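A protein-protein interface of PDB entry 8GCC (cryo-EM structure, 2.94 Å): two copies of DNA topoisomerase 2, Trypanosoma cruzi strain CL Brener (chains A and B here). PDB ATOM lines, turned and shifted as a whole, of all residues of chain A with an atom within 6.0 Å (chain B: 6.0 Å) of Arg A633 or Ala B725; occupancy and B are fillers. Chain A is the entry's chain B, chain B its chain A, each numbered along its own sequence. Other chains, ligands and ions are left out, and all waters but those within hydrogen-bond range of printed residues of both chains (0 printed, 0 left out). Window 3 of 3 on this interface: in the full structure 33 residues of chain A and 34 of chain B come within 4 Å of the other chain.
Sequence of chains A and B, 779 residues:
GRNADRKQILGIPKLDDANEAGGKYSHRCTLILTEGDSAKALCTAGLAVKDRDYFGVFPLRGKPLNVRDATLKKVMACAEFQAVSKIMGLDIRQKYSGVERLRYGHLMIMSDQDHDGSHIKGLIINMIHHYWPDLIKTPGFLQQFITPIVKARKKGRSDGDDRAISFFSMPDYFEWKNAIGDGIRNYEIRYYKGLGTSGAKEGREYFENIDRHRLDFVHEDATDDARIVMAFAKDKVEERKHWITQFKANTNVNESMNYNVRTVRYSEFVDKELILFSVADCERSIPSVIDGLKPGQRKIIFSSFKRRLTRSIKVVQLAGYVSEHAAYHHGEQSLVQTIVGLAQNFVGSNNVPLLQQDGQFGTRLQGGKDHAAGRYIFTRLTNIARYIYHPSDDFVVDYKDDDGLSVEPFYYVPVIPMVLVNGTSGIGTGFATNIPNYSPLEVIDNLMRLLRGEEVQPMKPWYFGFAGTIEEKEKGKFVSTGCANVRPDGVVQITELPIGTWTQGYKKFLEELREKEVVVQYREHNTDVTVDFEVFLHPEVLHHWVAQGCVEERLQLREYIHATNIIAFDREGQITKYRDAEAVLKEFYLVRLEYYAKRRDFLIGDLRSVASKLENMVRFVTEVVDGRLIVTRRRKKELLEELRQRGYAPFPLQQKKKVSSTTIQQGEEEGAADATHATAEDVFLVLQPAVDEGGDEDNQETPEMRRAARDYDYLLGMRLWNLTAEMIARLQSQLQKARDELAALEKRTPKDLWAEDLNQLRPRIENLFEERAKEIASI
The backbone carbonyl oxygen (O) of Leu B723 lies within hydrogen-bond range of the backbone NH (N) of Arg A633 (3.5 Å).
The backbone carbonyl oxygen (O) of Val A631 lies close to the backbone carbonyl oxygen (O) of Leu B723 (2.8 Å).
O of Val A631 touches CG2 of Thr B724, at 3.9 Å.
Thr A632 touches Val B625 (CB to CG2, 3.99 Å).
CA of Thr A632 touches O of Leu B723 (3.4 Å).
Arg A633 touches Ala B725 (CA to N, 3.9 Å).
O of Arg A634 touches CG2 of Thr B724, 3.1 Å away.
Arg A634 touches Ala B725 (O to N, 3.7 Å).
No position is printed for both chains.
Of the 8 pairs that touch across the chains among the printed residues, none has its exchanged pair printed and touching as well.
The backbone carbonyl oxygen (O) of Ile A630 lies within hydrogen-bond range of the guanidinium group (NH1) of Arg A634 (2.9 Å).
Printed residues of chain A that touch a printed residue of chain B: Val A631, Thr A632, Arg A633 and Arg A634.
Hydrophobic or aromatic side chains of chain A within 4 Å of the printed part of chain B: Val A631.
Of the 10 printed residues of chain B, 4 touch a printed residue of chain A.
Hydrophobic or aromatic side chains of chain B within 4 Å of the printed part of chain A: Val B625.
Among the printed residues, no Asp or Glu carboxylate lies within 4 Å of a Lys or Arg side-chain nitrogen of the other chain.
Ala B725 touches just these residues of chain A: Arg A633 (3.9 Å) and Arg A634 (3.7 Å).
Printed residues of chain B within 4 Å of Arg A634: Thr B724 (3.1 Å) and Ala B725 (3.7 Å).
Of the printed residues of chain B, Thr A632 touches Val B625 (3.99 Å) and Leu B723 (3.4 Å).
Printed residues of chain A within 4 Å of Val B625: Thr A632 (3.99 Å).
Printed residues of chain B within 4 Å of Val A631: Leu B723 (2.8 Å) and Thr B724 (3.9 Å).
Of the printed residues of chain A, Thr B724 touches Val A631 and Arg A634.
Met B727 touches none of the printed residues of chain A.
The nearest residue of chain A that does not touch Ala B725 is Arg A635 (4.8 Å).
The nearest printed residue of chain B that does not touch Thr A632 is Thr B724 (5.2 Å).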
ATOM      1  N   ILE A 630      13.766   3.397  10.065  1.00  0.00           N
ATOM      2  CA  ILE A 630      13.061   4.179  11.074  1.00  0.00           C
ATOM      3  C   ILE A 630      11.621   4.367  10.623  1.00  0.00           C
ATOM      4  O   ILE A 630      11.369   4.842   9.510  1.00  0.00           O
ATOM      5  CB  ILE A 630      13.740   5.539  11.322  1.00  0.00           C
ATOM      6  CG1 ILE A 630      13.775   6.374  10.040  1.00  0.00           C
ATOM      7  CG2 ILE A 630      15.146   5.339  11.863  1.00  0.00           C
ATOM      8  CD1 ILE A 630      12.801   7.525  10.045  1.00  0.00           C
ATOM      9  N   VAL A 631      10.683   3.997  11.490  1.00  0.00           N
ATOM     10  CA  VAL A 631       9.263   4.096  11.185  1.00  0.00           C
ATOM     11  C   VAL A 631       8.591   5.259  11.903  1.00  0.00           C
ATOM     12  O   VAL A 631       7.544   5.731  11.431  1.00  0.00           O
ATOM     13  CB  VAL A 631       8.536   2.776  11.518  1.00  0.00           C
ATOM     14  CG1 VAL A 631       7.033   2.940  11.375  1.00  0.00           C
ATOM     15  CG2 VAL A 631       9.041   1.657  10.628  1.00  0.00           C
ATOM     16  N   THR A 632       9.152   5.743  13.007  1.00  0.00           N
ATOM     17  CA  THR A 632       8.495   6.782  13.787  1.00  0.00           C
ATOM     18  C   THR A 632       8.293   8.037  12.948  1.00  0.00           C
ATOM     19  O   THR A 632       9.230   8.544  12.327  1.00  0.00           O
ATOM     20  CB  THR A 632       9.324   7.108  15.028  1.00  0.00           C
ATOM     21  OG1 THR A 632      10.597   7.629  14.633  1.00  0.00           O
ATOM     22  CG2 THR A 632       9.533   5.864  15.873  1.00  0.00           C
ATOM     23  N   ARG A 633       7.063   8.542  12.945  1.00  0.00           N
ATOM     24  CA  ARG A 633       6.707   9.771  12.241  1.00  0.00           C
ATOM     25  C   ARG A 633       7.193   9.728  10.793  1.00  0.00           C
ATOM     26  O   ARG A 633       8.011  10.537  10.353  1.00  0.00           O
ATOM     27  CB  ARG A 633       7.265  10.992  12.972  1.00  0.00           C
ATOM     28  N   ARG A 634       6.669   8.755  10.050  1.00  0.00           N
ATOM     29  CA  ARG A 634       6.992   8.579   8.641  1.00  0.00           C
ATOM     30  C   ARG A 634       5.701   8.499   7.841  1.00  0.00           C
ATOM     31  O   ARG A 634       4.795   7.742   8.199  1.00  0.00           O
ATOM     32  CB  ARG A 634       7.829   7.316   8.419  1.00  0.00           C
ATOM     33  CG  ARG A 634       9.274   7.445   8.875  1.00  0.00           C
ATOM     34  CD  ARG A 634      10.078   8.348   7.952  1.00  0.00           C
ATOM     35  NE  ARG A 634      10.063   7.877   6.572  1.00  0.00           N
ATOM     36  CZ  ARG A 634      10.733   6.820   6.135  1.00  0.00           C
ATOM     37  NH1 ARG A 634      11.492   6.098   6.944  1.00  0.00           N
ATOM     38  NH2 ARG A 634      10.640   6.478   4.854  1.00  0.00           N
ATOM     39  N   ARG A 635       5.625   9.270   6.761  1.00  0.00           N
ATOM     40  CA  ARG A 635       4.443   9.236   5.914  1.00  0.00           C
ATOM     41  C   ARG A 635       4.252   7.837   5.343  1.00  0.00           C
ATOM     42  O   ARG A 635       5.215   7.124   5.050  1.00  0.00           O
ATOM     43  CB  ARG A 635       4.567  10.258   4.783  1.00  0.00           C
ATOM     44  N   VAL B 625       7.617   7.754  20.075  1.00  0.00           N
ATOM     45  CA  VAL B 625       8.139   8.444  18.900  1.00  0.00           C
ATOM     46  C   VAL B 625       9.143   9.512  19.311  1.00  0.00           C
ATOM     47  O   VAL B 625      10.207   9.656  18.696  1.00  0.00           O
ATOM     48  CB  VAL B 625       6.985   9.041  18.079  1.00  0.00           C
ATOM     49  CG1 VAL B 625       7.512  10.055  17.074  1.00  0.00           C
ATOM     50  CG2 VAL B 625       6.216   7.937  17.382  1.00  0.00           C
ATOM     51  N   ASN B 722       0.695   2.357  14.099  1.00  0.00           N
ATOM     52  CA  ASN B 722       0.368   3.517  14.916  1.00  0.00           C
ATOM     53  C   ASN B 722       1.554   4.448  15.119  1.00  0.00           C
ATOM     54  O   ASN B 722       1.355   5.589  15.544  1.00  0.00           O
ATOM     55  CB  ASN B 722      -0.171   3.062  16.270  1.00  0.00           C
ATOM     56  CG  ASN B 722      -1.437   2.244  16.143  1.00  0.00           C
ATOM     57  OD1 ASN B 722      -2.520   2.784  15.933  1.00  0.00           O
ATOM     58  ND2 ASN B 722      -1.307   0.932  16.269  1.00  0.00           N
ATOM     59  N   LEU B 723       2.772   3.995  14.836  1.00  0.00           N
ATOM     60  CA  LEU B 723       3.957   4.846  14.955  1.00  0.00           C
ATOM     61  C   LEU B 723       4.266   5.548  13.636  1.00  0.00           C
ATOM     62  O   LEU B 723       5.387   5.521  13.135  1.00  0.00           O
ATOM     63  CB  LEU B 723       5.143   4.016  15.427  1.00  0.00           C
ATOM     64  CG  LEU B 723       5.291   3.882  16.942  1.00  0.00           C
ATOM     65  CD1 LEU B 723       4.015   3.347  17.563  1.00  0.00           C
ATOM     66  CD2 LEU B 723       6.470   2.988  17.280  1.00  0.00           C
ATOM     67  N   THR B 724       3.253   6.198  13.072  1.00  0.00           N
ATOM     68  CA  THR B 724       3.385   6.921  11.817  1.00  0.00           C
ATOM     69  C   THR B 724       2.646   8.245  11.944  1.00  0.00           C
ATOM     70  O   THR B 724       1.738   8.393  12.764  1.00  0.00           O
ATOM     71  CB  THR B 724       2.829   6.119  10.630  1.00  0.00           C
ATOM     72  OG1 THR B 724       1.856   5.179  11.097  1.00  0.00           O
ATOM     73  CG2 THR B 724       3.939   5.366   9.921  1.00  0.00           C
ATOM     74  N   ALA B 725       3.045   9.214  11.120  1.00  0.00           N
ATOM     75  CA  ALA B 725       2.444  10.541  11.210  1.00  0.00           C
ATOM     76  C   ALA B 725       0.937  10.475  11.002  1.00  0.00           C
ATOM     77  O   ALA B 725       0.161  10.999  11.813  1.00  0.00           O
ATOM     78  CB  ALA B 725       3.090  11.474  10.186  1.00  0.00           C
ATOM     79  N   GLU B 726       0.501   9.819   9.926  1.00  0.00           N
ATOM     80  CA  GLU B 726      -0.924   9.750   9.632  1.00  0.00           C
ATOM     81  C   GLU B 726      -1.680   9.043  10.747  1.00  0.00           C
ATOM     82  O   GLU B 726      -2.735   9.509  11.194  1.00  0.00           O
ATOM     83  CB  GLU B 726      -1.146   9.038   8.297  1.00  0.00           C
ATOM     84  N   MET B 727      -1.148   7.917  11.223  1.00  0.00           N
ATOM     85  CA  MET B 727      -1.855   7.157  12.246  1.00  0.00           C
ATOM     86  C   MET B 727      -1.802   7.849  13.600  1.00  0.00           C
ATOM     87  O   MET B 727      -2.755   7.755  14.376  1.00  0.00           O
ATOM     88  CB  MET B 727      -1.278   5.747  12.343  1.00  0.00           C
ATOM     89  CG  MET B 727      -1.857   4.771  11.324  1.00  0.00           C
ATOM     90  SD  MET B 727      -3.587   4.298  11.555  1.00  0.00           S
ATOM     91  CE  MET B 727      -3.914   4.745  13.258  1.00  0.00           C
ATOM     92  N   ILE B 728      -0.710   8.551  13.904  1.00  0.00           N
ATOM     93  CA  ILE B 728      -0.668   9.335  15.136  1.00  0.00           C
ATOM     94  C   ILE B 728      -1.728  10.427  15.101  1.00  0.00           C
ATOM     95  O   ILE B 728      -2.447  10.653  16.085  1.00  0.00           O
ATOM     96  CB  ILE B 728       0.738   9.925  15.349  1.00  0.00           C
ATOM     97  CG1 ILE B 728       1.736   8.819  15.675  1.00  0.00           C
ATOM     98  CG2 ILE B 728       0.715  10.941  16.471  1.00  0.00           C
ATOM     99  CD1 ILE B 728       3.174   9.212  15.435  1.00  0.00           C
ATOM    100  N   ALA B 729      -1.842  11.124  13.969  1.00  0.00           N
ATOM    101  CA  ALA B 729      -2.870  12.151  13.842  1.00  0.00           C
ATOM    102  C   ALA B 729      -4.263  11.549  13.961  1.00  0.00           C
ATOM    103  O   ALA B 729      -5.148  12.131  14.597  1.00  0.00           O
ATOM    104  CB  ALA B 729      -2.715  12.885  12.512  1.00  0.00           C
ATOM    105  N   ARG B 730      -4.478  10.382  13.349  1.00  0.00           N
ATOM    106  CA  ARG B 730      -5.781   9.732  13.451  1.00  0.00           C
ATOM    107  C   ARG B 730      -6.093   9.348  14.892  1.00  0.00           C
ATOM    108  O   ARG B 730      -7.235   9.472  15.340  1.00  0.00           O
ATOM    109  CB  ARG B 730      -5.831   8.502  12.548  1.00  0.00           C
ATOM    110  CG  ARG B 730      -6.957   7.535  12.887  1.00  0.00           C
ATOM    111  CD  ARG B 730      -7.467   6.795  11.661  1.00  0.00           C
ATOM    112  NE  ARG B 730      -6.403   6.463  10.720  1.00  0.00           N
ATOM    113  CZ  ARG B 730      -6.582   5.768   9.605  1.00  0.00           C
ATOM    114  NH1 ARG B 730      -7.774   5.311   9.257  1.00  0.00           N
ATOM    115  NH2 ARG B 730      -5.539   5.527   8.817  1.00  0.00           N
